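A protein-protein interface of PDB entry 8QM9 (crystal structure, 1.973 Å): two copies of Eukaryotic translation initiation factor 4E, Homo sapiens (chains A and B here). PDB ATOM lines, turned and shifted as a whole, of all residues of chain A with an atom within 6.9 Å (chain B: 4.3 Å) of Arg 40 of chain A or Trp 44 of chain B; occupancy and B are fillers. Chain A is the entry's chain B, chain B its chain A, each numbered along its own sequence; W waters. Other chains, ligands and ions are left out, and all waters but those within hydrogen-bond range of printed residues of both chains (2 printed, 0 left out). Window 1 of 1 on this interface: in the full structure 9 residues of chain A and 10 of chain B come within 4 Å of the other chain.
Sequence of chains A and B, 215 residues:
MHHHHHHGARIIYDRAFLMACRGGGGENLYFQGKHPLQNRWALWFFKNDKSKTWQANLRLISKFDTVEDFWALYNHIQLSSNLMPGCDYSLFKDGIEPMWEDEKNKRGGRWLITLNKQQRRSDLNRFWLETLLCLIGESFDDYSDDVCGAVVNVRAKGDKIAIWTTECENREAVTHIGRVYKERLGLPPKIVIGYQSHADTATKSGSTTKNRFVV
The backbone NH (N) of Leu 60 of chain B sits at hydrogen-bond distance from the side-chain carboxylate (OD2) of Asp 94 of chain A, 3.0 Å away.
The guanidinium group of Arg 40 of chain A lies within hydrogen-bond range of the backbone carbonyl oxygen of Leu 58 of chain B, 3.1 Å away.
NH2 of Arg 40 of chain A is in salt-bridge range of OE1 of Glu 97 of chain B, 3.2 Å away.
The backbone carbonyl oxygen (O) of Leu 58 of chain B sits at hydrogen-bond distance from the side-chain amino group (NZ) of Lys 63 of chain A (3.0 Å).
NZ of Lys 63 of chain A is in salt-bridge range of OD1 of Asp 94 of chain A (2.8 Å).
N of Leu 37 of chain A is in hydrogen-bond range of O of Asp 65 of chain A (2.8 Å).
O of Phe 45 of chain B lies within hydrogen-bond range of N of Arg 59 of chain B (2.8 Å).
NH1 of Arg 40 of chain A is in salt-bridge range of OD2 of Asp 94 of chain A (2.7 Å).
N of Trp 44 of chain B sits at hydrogen-bond distance from O of Ser 90 of chain B (2.8 Å).
Among the printed residues, merely in contact across the chains: Arg 40 of chain A with Trp 44 of chain B (3.3 Å), Arg 40 of chain A with Arg 59 of chain B (3.96 Å), Arg 40 of chain A with Leu 60 of chain B (3.8 Å), Asp 65 of chain A with Trp 44 of chain B (3.7 Å) and Asp 94 of chain A with Arg 59 of chain B (3.6 Å).
Of chain B, only Trp 44 (3.3 Å), Leu 58 (3.1 Å), Arg 59 (3.96 Å), Leu 60 (3.8 Å) and Glu 97 (3.2 Å) come within 4 Å of Arg 40 of chain A.
Printed residues of chain B within 4 Å of Asp 65 of chain A: Trp 44 (3.7 Å).
Of the printed residues of chain B, Asp 94 of chain A touches Arg 59 (3.6 Å) and Leu 60 (3.0 Å).
Trp 44 of chain B touches two residues of chain A.
Printed residues of chain A within 4 Å of Leu 58 of chain B: Arg 40 and Lys 63.
Of the printed residues of chain A, Arg 59 of chain B touches Arg 40 (3.96 Å) and Asp 94 (3.6 Å).
Of the printed residues of chain A, Leu 60 of chain B touches Arg 40 (3.8 Å) and Asp 94 (3.0 Å).
Phe 92 of chain B touches none of the printed residues of chain A.
The nearest printed residue of chain B that does not touch Arg 40 of chain A is Pro 98 of chain B (6.7 Å).
The nearest printed residue of chain A that does not touch Glu 97 of chain B is Lys 63 of chain A (4.4 Å).
Of the 14 printed residues of chain B, 5 touch a printed residue of chain A.
Printed residues of chain A that touch a printed residue of chain B: Arg 40, Lys 63, Asp 65 and Asp 94.
Among the printed residues, 9 pairs touch across the chains.
Positions printed for both chains: 42 and 92.
Water W2 lies within hydrogen-bond range of the guanidinium group of Arg 40 of chain A (2.5 Å), the side-chain carboxylate of Glu 97 of chain B (2.7 Å) and the side-chain carboxylate of Asp 65 of chain A (3.3 Å).
Water W1 bridges NZ of Lys 63 of chain A (3.1 Å) and NE of Arg 59 of chain B (3.5 Å).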
ATOM      1  N   LEU A  37      -9.998 -16.500  27.781  1.00  0.00           N
ATOM      2  CA  LEU A  37     -11.136 -16.090  26.960  1.00  0.00           C
ATOM      3  C   LEU A  37     -11.458 -17.197  25.957  1.00  0.00           C
ATOM      4  O   LEU A  37     -10.588 -17.966  25.561  1.00  0.00           O
ATOM      5  CB  LEU A  37     -10.833 -14.760  26.248  1.00  0.00           C
ATOM      6  CG  LEU A  37     -10.470 -13.542  27.134  1.00  0.00           C
ATOM      7  CD1 LEU A  37     -10.216 -12.257  26.266  1.00  0.00           C
ATOM      8  CD2 LEU A  37     -11.513 -13.267  28.163  1.00  0.00           C
ATOM      9  N   GLN A  38     -12.725 -17.302  25.572  1.00  0.00           N
ATOM     10  CA  GLN A  38     -13.166 -18.213  24.513  1.00  0.00           C
ATOM     11  C   GLN A  38     -12.420 -17.966  23.208  1.00  0.00           C
ATOM     12  O   GLN A  38     -12.131 -18.908  22.467  1.00  0.00           O
ATOM     13  CB  GLN A  38     -14.684 -18.013  24.268  1.00  0.00           C
ATOM     14  CG  GLN A  38     -15.288 -18.874  23.146  1.00  0.00           C
ATOM     15  CD  GLN A  38     -15.355 -20.321  23.512  1.00  0.00           C
ATOM     16  OE1 GLN A  38     -15.184 -20.724  24.677  1.00  0.00           O
ATOM     17  NE2 GLN A  38     -15.612 -21.139  22.494  1.00  0.00           N
ATOM     18  N   ASN A  39     -12.138 -16.684  22.923  1.00  0.00           N
ATOM     19  CA  ASN A  39     -11.474 -16.196  21.725  1.00  0.00           C
ATOM     20  C   ASN A  39     -10.251 -15.353  22.077  1.00  0.00           C
ATOM     21  O   ASN A  39     -10.194 -14.731  23.157  1.00  0.00           O
ATOM     22  CB  ASN A  39     -12.432 -15.345  20.942  1.00  0.00           C
ATOM     23  CG  ASN A  39     -13.484 -16.170  20.279  1.00  0.00           C
ATOM     24  OD1 ASN A  39     -13.164 -17.044  19.490  1.00  0.00           O
ATOM     25  ND2 ASN A  39     -14.712 -15.950  20.549  1.00  0.00           N
ATOM     26  N   ARG A  40      -9.256 -15.359  21.173  1.00  0.00           N
ATOM     27  CA  ARG A  40      -8.218 -14.349  21.130  1.00  0.00           C
ATOM     28  C   ARG A  40      -8.716 -13.125  20.347  1.00  0.00           C
ATOM     29  O   ARG A  40      -9.423 -13.264  19.347  1.00  0.00           O
ATOM     30  CB  ARG A  40      -6.964 -14.914  20.480  1.00  0.00           C
ATOM     31  CG  ARG A  40      -5.722 -14.014  20.559  1.00  0.00           C
ATOM     32  CD  ARG A  40      -4.470 -14.899  20.654  1.00  0.00           C
ATOM     33  NE  ARG A  40      -3.221 -14.123  20.718  1.00  0.00           N
ATOM     34  CZ  ARG A  40      -2.436 -13.816  19.686  1.00  0.00           C
ATOM     35  NH1 ARG A  40      -2.735 -14.237  18.459  1.00  0.00           N
ATOM     36  NH2 ARG A  40      -1.324 -13.115  19.878  1.00  0.00           N
ATOM     37  N   TRP A  41      -8.337 -11.923  20.824  1.00  0.00           N
ATOM     38  CA  TRP A  41      -8.859 -10.662  20.339  1.00  0.00           C
ATOM     39  C   TRP A  41      -7.710  -9.769  20.008  1.00  0.00           C
ATOM     40  O   TRP A  41      -6.678  -9.797  20.690  1.00  0.00           O
ATOM     41  CB  TRP A  41      -9.728  -9.938  21.398  1.00  0.00           C
ATOM     42  CG  TRP A  41     -10.939 -10.714  21.784  1.00  0.00           C
ATOM     43  CD1 TRP A  41     -11.005 -11.703  22.720  1.00  0.00           C
ATOM     44  CD2 TRP A  41     -12.223 -10.687  21.136  1.00  0.00           C
ATOM     45  NE1 TRP A  41     -12.244 -12.298  22.700  1.00  0.00           N
ATOM     46  CE2 TRP A  41     -13.025 -11.670  21.753  1.00  0.00           C
ATOM     47  CE3 TRP A  41     -12.766  -9.946  20.085  1.00  0.00           C
ATOM     48  CZ2 TRP A  41     -14.345 -11.900  21.364  1.00  0.00           C
ATOM     49  CZ3 TRP A  41     -14.073 -10.159  19.724  1.00  0.00           C
ATOM     50  CH2 TRP A  41     -14.848 -11.128  20.360  1.00  0.00           C
ATOM     51  N   ALA A  42      -7.896  -8.961  18.956  1.00  0.00           N
ATOM     52  CA  ALA A  42      -6.889  -8.025  18.502  1.00  0.00           C
ATOM     53  C   ALA A  42      -7.453  -6.620  18.540  1.00  0.00           C
ATOM     54  O   ALA A  42      -8.553  -6.366  18.056  1.00  0.00           O
ATOM     55  CB  ALA A  42      -6.443  -8.398  17.095  1.00  0.00           C
ATOM     56  N   SER A  62      -2.300  -4.566  19.798  1.00  0.00           N
ATOM     57  CA  SER A  62      -2.047  -5.642  20.752  1.00  0.00           C
ATOM     58  C   SER A  62      -3.057  -6.770  20.609  1.00  0.00           C
ATOM     59  O   SER A  62      -4.167  -6.547  20.121  1.00  0.00           O
ATOM     60  CB  SER A  62      -2.128  -5.075  22.174  1.00  0.00           C
ATOM     61  OG  SER A  62      -1.385  -5.829  23.112  1.00  0.00           O
ATOM     62  N   LYS A  63      -2.683  -7.983  21.048  1.00  0.00           N
ATOM     63  CA  LYS A  63      -3.609  -9.102  21.137  1.00  0.00           C
ATOM     64  C   LYS A  63      -3.641  -9.683  22.542  1.00  0.00           C
ATOM     65  O   LYS A  63      -2.698  -9.532  23.278  1.00  0.00           O
ATOM     66  CB  LYS A  63      -3.221 -10.199  20.155  1.00  0.00           C
ATOM     67  CG  LYS A  63      -3.187  -9.726  18.718  1.00  0.00           C
ATOM     68  CD  LYS A  63      -3.221 -10.884  17.731  1.00  0.00           C
ATOM     69  CE  LYS A  63      -3.073 -10.413  16.320  1.00  0.00           C
ATOM     70  NZ  LYS A  63      -2.784 -11.544  15.428  1.00  0.00           N
ATOM     71  N   PHE A  64      -4.723 -10.371  22.901  1.00  0.00           N
ATOM     72  CA  PHE A  64      -4.862 -10.956  24.228  1.00  0.00           C
ATOM     73  C   PHE A  64      -5.894 -12.061  24.205  1.00  0.00           C
ATOM     74  O   PHE A  64      -6.741 -12.122  23.323  1.00  0.00           O
ATOM     75  CB  PHE A  64      -5.200  -9.889  25.283  1.00  0.00           C
ATOM     76  CG  PHE A  64      -6.503  -9.170  25.011  1.00  0.00           C
ATOM     77  CD1 PHE A  64      -7.706  -9.682  25.465  1.00  0.00           C
ATOM     78  CD2 PHE A  64      -6.527  -8.013  24.274  1.00  0.00           C
ATOM     79  CE1 PHE A  64      -8.898  -9.039  25.190  1.00  0.00           C
ATOM     80  CE2 PHE A  64      -7.717  -7.386  23.981  1.00  0.00           C
ATOM     81  CZ  PHE A  64      -8.897  -7.883  24.463  1.00  0.00           C
ATOM     82  N   ASP A  65      -5.826 -12.946  25.193  1.00  0.00           N
ATOM     83  CA  ASP A  65      -6.762 -14.051  25.311  1.00  0.00           C
ATOM     84  C   ASP A  65      -7.021 -14.473  26.746  1.00  0.00           C
ATOM     85  O   ASP A  65      -7.420 -15.611  26.981  1.00  0.00           O
ATOM     86  CB  ASP A  65      -6.316 -15.216  24.434  1.00  0.00           C
ATOM     87  CG  ASP A  65      -4.968 -15.829  24.749  1.00  0.00           C
ATOM     88  OD1 ASP A  65      -4.237 -15.263  25.565  1.00  0.00           O
ATOM     89  OD2 ASP A  65      -4.651 -16.871  24.168  1.00  0.00           O
ATOM     90  N   THR A  66      -6.816 -13.564  27.707  1.00  0.00           N
ATOM     91  CA  THR A  66      -7.242 -13.737  29.076  1.00  0.00           C
ATOM     92  C   THR A  66      -7.945 -12.448  29.539  1.00  0.00           C
ATOM     93  O   THR A  66      -7.727 -11.360  28.978  1.00  0.00           O
ATOM     94  CB  THR A  66      -6.079 -14.086  30.011  1.00  0.00           C
ATOM     95  OG1 THR A  66      -5.301 -12.915  30.271  1.00  0.00           O
ATOM     96  CG2 THR A  66      -5.213 -15.221  29.497  1.00  0.00           C
ATOM     97  N   PHE A  92     -11.337  -6.973  17.343  1.00  0.00           N
ATOM     98  CA  PHE A  92     -11.856  -8.040  16.467  1.00  0.00           C
ATOM     99  C   PHE A  92     -11.239  -9.327  16.831  1.00  0.00           C
ATOM    100  O   PHE A  92     -10.122  -9.364  17.330  1.00  0.00           O
ATOM    101  CB  PHE A  92     -11.591  -7.752  14.972  1.00  0.00           C
ATOM    102  CG  PHE A  92     -12.656  -6.893  14.328  1.00  0.00           C
ATOM    103  CD1 PHE A  92     -12.801  -5.562  14.683  1.00  0.00           C
ATOM    104  CD2 PHE A  92     -13.533  -7.426  13.407  1.00  0.00           C
ATOM    105  CE1 PHE A  92     -13.814  -4.793  14.137  1.00  0.00           C
ATOM    106  CE2 PHE A  92     -14.533  -6.649  12.849  1.00  0.00           C
ATOM    107  CZ  PHE A  92     -14.674  -5.345  13.220  1.00  0.00           C
ATOM    108  N   LYS A  93     -11.967 -10.436  16.600  1.00  0.00           N
ATOM    109  CA  LYS A  93     -11.402 -11.761  16.810  1.00  0.00           C
ATOM    110  C   LYS A  93     -10.125 -11.931  15.964  1.00  0.00           C
ATOM    111  O   LYS A  93      -9.986 -11.400  14.857  1.00  0.00           O
ATOM    112  CB  LYS A  93     -12.407 -12.869  16.520  1.00  0.00           C
ATOM    113  CG  LYS A  93     -13.566 -12.904  17.459  1.00  0.00           C
ATOM    114  CD  LYS A  93     -14.633 -13.840  16.998  1.00  0.00           C
ATOM    115  CE  LYS A  93     -15.681 -14.043  18.057  1.00  0.00           C
ATOM    116  NZ  LYS A  93     -16.810 -14.824  17.533  1.00  0.00           N
ATOM    117  N   ASP A  94      -9.190 -12.667  16.524  1.00  0.00           N
ATOM    118  CA  ASP A  94      -7.906 -12.951  15.896  1.00  0.00           C
ATOM    119  C   ASP A  94      -8.142 -13.570  14.506  1.00  0.00           C
ATOM    120  O   ASP A  94      -8.887 -14.544  14.395  1.00  0.00           O
ATOM    121  CB  ASP A  94      -7.106 -13.897  16.813  1.00  0.00           C
ATOM    122  CG  ASP A  94      -5.612 -14.006  16.553  1.00  0.00           C
ATOM    123  OD1 ASP A  94      -5.065 -13.139  15.846  1.00  0.00           O
ATOM    124  OD2 ASP A  94      -4.992 -14.947  17.075  1.00  0.00           O
ATOM    125  N   GLY A  95      -7.563 -12.926  13.488  1.00  0.00           N
ATOM    126  CA  GLY A  95      -7.636 -13.358  12.105  1.00  0.00           C
ATOM    127  C   GLY A  95      -8.730 -12.721  11.278  1.00  0.00           C
ATOM    128  O   GLY A  95      -8.915 -13.120  10.133  1.00  0.00           O
ATOM    129  N   ALA B  42      -3.038 -24.771  23.571  1.00  0.00           N
ATOM    130  CA  ALA B  42      -3.362 -23.910  22.466  1.00  0.00           C
ATOM    131  C   ALA B  42      -2.367 -24.116  21.348  1.00  0.00           C
ATOM    132  O   ALA B  42      -1.164 -24.129  21.585  1.00  0.00           O
ATOM    133  CB  ALA B  42      -3.359 -22.458  22.946  1.00  0.00           C
ATOM    134  N   LEU B  43      -2.867 -24.306  20.109  1.00  0.00           N
ATOM    135  CA  LEU B  43      -2.062 -24.408  18.909  1.00  0.00           C
ATOM    136  C   LEU B  43      -1.959 -23.055  18.268  1.00  0.00           C
ATOM    137  O   LEU B  43      -2.994 -22.459  18.015  1.00  0.00           O
ATOM    138  CB  LEU B  43      -2.704 -25.359  17.915  1.00  0.00           C
ATOM    139  CG  LEU B  43      -1.996 -25.493  16.556  1.00  0.00           C
ATOM    140  CD1 LEU B  43      -0.530 -25.854  16.718  1.00  0.00           C
ATOM    141  CD2 LEU B  43      -2.787 -26.459  15.639  1.00  0.00           C
ATOM    142  N   TRP B  44      -0.738 -22.582  17.992  1.00  0.00           N
ATOM    143  CA  TRP B  44      -0.423 -21.315  17.347  1.00  0.00           C
ATOM    144  C   TRP B  44       0.308 -21.521  16.027  1.00  0.00           C
ATOM    145  O   TRP B  44       1.056 -22.491  15.872  1.00  0.00           O
ATOM    146  CB  TRP B  44       0.488 -20.478  18.251  1.00  0.00           C
ATOM    147  CG  TRP B  44      -0.031 -20.270  19.633  1.00  0.00           C
ATOM    148  CD1 TRP B  44       0.021 -21.131  20.680  1.00  0.00           C
ATOM    149  CD2 TRP B  44      -0.705 -19.107  20.109  1.00  0.00           C
ATOM    150  NE1 TRP B  44      -0.536 -20.556  21.793  1.00  0.00           N
ATOM    151  CE2 TRP B  44      -0.988 -19.311  21.472  1.00  0.00           C
ATOM    152  CE3 TRP B  44      -1.035 -17.883  19.531  1.00  0.00           C
ATOM    153  CZ2 TRP B  44      -1.636 -18.361  22.241  1.00  0.00           C
ATOM    154  CZ3 TRP B  44      -1.672 -16.952  20.292  1.00  0.00           C
ATOM    155  CH2 TRP B  44      -1.941 -17.174  21.638  1.00  0.00           C
ATOM    156  N   PHE B  45       0.097 -20.581  15.077  1.00  0.00           N
ATOM    157  CA  PHE B  45       0.818 -20.461  13.802  1.00  0.00           C
ATOM    158  C   PHE B  45       1.470 -19.083  13.744  1.00  0.00           C
ATOM    159  O   PHE B  45       0.879 -18.090  14.172  1.00  0.00           O
ATOM    160  CB  PHE B  45      -0.181 -20.606  12.645  1.00  0.00           C
ATOM    161  CG  PHE B  45       0.371 -20.420  11.269  1.00  0.00           C
ATOM    162  CD1 PHE B  45       1.228 -21.355  10.716  1.00  0.00           C
ATOM    163  CD2 PHE B  45       0.033 -19.311  10.512  1.00  0.00           C
ATOM    164  CE1 PHE B  45       1.752 -21.172   9.449  1.00  0.00           C
ATOM    165  CE2 PHE B  45       0.563 -19.134   9.235  1.00  0.00           C
ATOM    166  CZ  PHE B  45       1.411 -20.066   8.711  1.00  0.00           C
ATOM    167  N   LEU B  58       1.449 -13.666  14.593  1.00  0.00           N
ATOM    168  CA  LEU B  58       1.141 -14.737  15.515  1.00  0.00           C
ATOM    169  C   LEU B  58      -0.355 -14.903  15.607  1.00  0.00           C
ATOM    170  O   LEU B  58      -1.087 -13.954  15.897  1.00  0.00           O
ATOM    171  CB  LEU B  58       1.818 -14.491  16.883  1.00  0.00           C
ATOM    172  CG  LEU B  58       1.713 -15.591  17.981  1.00  0.00           C
ATOM    173  CD1 LEU B  58       2.242 -16.985  17.510  1.00  0.00           C
ATOM    174  CD2 LEU B  58       2.476 -15.168  19.279  1.00  0.00           C
ATOM    175  N   ARG B  59      -0.828 -16.132  15.334  1.00  0.00           N
ATOM    176  CA  ARG B  59      -2.258 -16.460  15.222  1.00  0.00           C
ATOM    177  C   ARG B  59      -2.557 -17.682  16.077  1.00  0.00           C
ATOM    178  O   ARG B  59      -1.810 -18.650  16.064  1.00  0.00           O
ATOM    179  CB  ARG B  59      -2.641 -16.796  13.780  1.00  0.00           C
ATOM    180  CG  ARG B  59      -2.126 -15.806  12.748  1.00  0.00           C
ATOM    181  CD  ARG B  59      -3.179 -14.793  12.276  1.00  0.00           C
ATOM    182  NE  ARG B  59      -2.565 -13.600  11.673  1.00  0.00           N
ATOM    183  CZ  ARG B  59      -1.979 -13.544  10.475  1.00  0.00           C
ATOM    184  NH1 ARG B  59      -1.903 -14.631   9.707  1.00  0.00           N
ATOM    185  NH2 ARG B  59      -1.460 -12.404  10.038  1.00  0.00           N
ATOM    186  N   LEU B  60      -3.643 -17.629  16.813  1.00  0.00           N
ATOM    187  CA  LEU B  60      -4.147 -18.774  17.552  1.00  0.00           C
ATOM    188  C   LEU B  60      -5.060 -19.535  16.626  1.00  0.00           C
ATOM    189  O   LEU B  60      -5.935 -18.910  16.028  1.00  0.00           O
ATOM    190  CB  LEU B  60      -4.918 -18.285  18.763  1.00  0.00           C
ATOM    191  CG  LEU B  60      -5.674 -19.345  19.532  1.00  0.00           C
ATOM    192  CD1 LEU B  60      -4.701 -20.195  20.320  1.00  0.00           C
ATOM    193  CD2 LEU B  60      -6.743 -18.705  20.420  1.00  0.00           C
ATOM    194  N   ASP B  88       6.122 -21.280  11.626  1.00  0.00           N
ATOM    195  CA  ASP B  88       6.335 -21.908  12.916  1.00  0.00           C
ATOM    196  C   ASP B  88       4.997 -22.310  13.460  1.00  0.00           C
ATOM    197  O   ASP B  88       4.021 -21.571  13.308  1.00  0.00           O
ATOM    198  CB  ASP B  88       6.998 -20.959  13.928  1.00  0.00           C
ATOM    199  CG  ASP B  88       8.229 -20.200  13.421  1.00  0.00           C
ATOM    200  OD1 ASP B  88       8.998 -20.781  12.611  1.00  0.00           O
ATOM    201  OD2 ASP B  88       8.422 -19.033  13.839  1.00  0.00           O
ATOM    202  N   TYR B  89       4.946 -23.494  14.078  1.00  0.00           N
ATOM    203  CA  TYR B  89       3.796 -23.961  14.839  1.00  0.00           C
ATOM    204  C   TYR B  89       4.229 -24.171  16.285  1.00  0.00           C
ATOM    205  O   TYR B  89       5.378 -24.569  16.558  1.00  0.00           O
ATOM    206  CB  TYR B  89       3.266 -25.283  14.302  1.00  0.00           C
ATOM    207  CG  TYR B  89       2.509 -25.171  13.006  1.00  0.00           C
ATOM    208  CD1 TYR B  89       3.165 -25.213  11.794  1.00  0.00           C
ATOM    209  CD2 TYR B  89       1.130 -25.015  12.996  1.00  0.00           C
ATOM    210  CE1 TYR B  89       2.468 -25.103  10.597  1.00  0.00           C
ATOM    211  CE2 TYR B  89       0.422 -24.927  11.807  1.00  0.00           C
ATOM    212  CZ  TYR B  89       1.098 -24.958  10.607  1.00  0.00           C
ATOM    213  OH  TYR B  89       0.412 -24.871   9.420  1.00  0.00           O
ATOM    214  N   SER B  90       3.319 -23.906  17.179  1.00  0.00           N
ATOM    215  CA  SER B  90       3.563 -24.033  18.614  1.00  0.00           C
ATOM    216  C   SER B  90       2.374 -24.592  19.332  1.00  0.00           C
ATOM    217  O   SER B  90       1.247 -24.189  19.055  1.00  0.00           O
ATOM    218  CB  SER B  90       3.915 -22.687  19.210  1.00  0.00           C
ATOM    219  OG  SER B  90       5.081 -22.173  18.607  1.00  0.00           O
ATOM    220  N   PHE B  92       1.249 -24.642  23.183  1.00  0.00           N
ATOM    221  CA  PHE B  92       1.601 -24.108  24.512  1.00  0.00           C
ATOM    222  C   PHE B  92       0.457 -24.254  25.424  1.00  0.00           C
ATOM    223  O   PHE B  92      -0.703 -24.246  24.985  1.00  0.00           O
ATOM    224  CB  PHE B  92       2.037 -22.624  24.456  1.00  0.00           C
ATOM    225  CG  PHE B  92       3.504 -22.414  24.135  1.00  0.00           C
ATOM    226  CD1 PHE B  92       4.009 -22.750  22.899  1.00  0.00           C
ATOM    227  CD2 PHE B  92       4.385 -21.976  25.107  1.00  0.00           C
ATOM    228  CE1 PHE B  92       5.361 -22.632  22.634  1.00  0.00           C
ATOM    229  CE2 PHE B  92       5.742 -21.841  24.835  1.00  0.00           C
ATOM    230  CZ  PHE B  92       6.222 -22.179  23.615  1.00  0.00           C
ATOM    231  N   ILE B  96      -0.136 -19.063  28.038  1.00  0.00           N
ATOM    232  CA  ILE B  96       1.264 -18.770  27.731  1.00  0.00           C
ATOM    233  C   ILE B  96       1.366 -18.503  26.228  1.00  0.00           C
ATOM    234  O   ILE B  96       1.075 -19.392  25.420  1.00  0.00           O
ATOM    235  CB  ILE B  96       2.209 -19.939  28.119  1.00  0.00           C
ATOM    236  CG1 ILE B  96       1.996 -20.390  29.590  1.00  0.00           C
ATOM    237  CG2 ILE B  96       3.669 -19.555  27.833  1.00  0.00           C
ATOM    238  CD1 ILE B  96       2.936 -21.579  30.036  1.00  0.00           C
ATOM    239  N   GLU B  97       1.777 -17.288  25.860  1.00  0.00           N
ATOM    240  CA  GLU B  97       2.087 -16.993  24.475  1.00  0.00           C
ATOM    241  C   GLU B  97       3.406 -17.657  24.062  1.00  0.00           C
ATOM    242  O   GLU B  97       4.312 -17.787  24.890  1.00  0.00           O
ATOM    243  CB  GLU B  97       2.111 -15.481  24.232  1.00  0.00           C
ATOM    244  CG  GLU B  97       0.718 -14.841  24.269  1.00  0.00           C
ATOM    245  CD  GLU B  97       0.680 -13.404  23.781  1.00  0.00           C
ATOM    246  OE1 GLU B  97      -0.149 -13.099  22.894  1.00  0.00           O
ATOM    247  OE2 GLU B  97       1.487 -12.584  24.279  1.00  0.00           O
ATOM    248  N   PRO B  98       3.525 -18.154  22.809  1.00  0.00           N
ATOM    249  CA  PRO B  98       4.778 -18.741  22.354  1.00  0.00           C
ATOM    250  C   PRO B  98       5.874 -17.764  22.024  1.00  0.00           C
ATOM    251  O   PRO B  98       6.493 -17.873  20.968  1.00  0.00           O
ATOM    252  CB  PRO B  98       4.334 -19.567  21.113  1.00  0.00           C
ATOM    253  CG  PRO B  98       3.265 -18.827  20.560  1.00  0.00           C
ATOM    254  CD  PRO B  98       2.480 -18.308  21.773  1.00  0.00           C
HETATM  255  O   HOH W   1      -3.232 -10.330  12.618  1.00  0.00           O
HETATM  256  O   HOH W   2      -2.811 -13.612  23.106  1.00  0.00           O
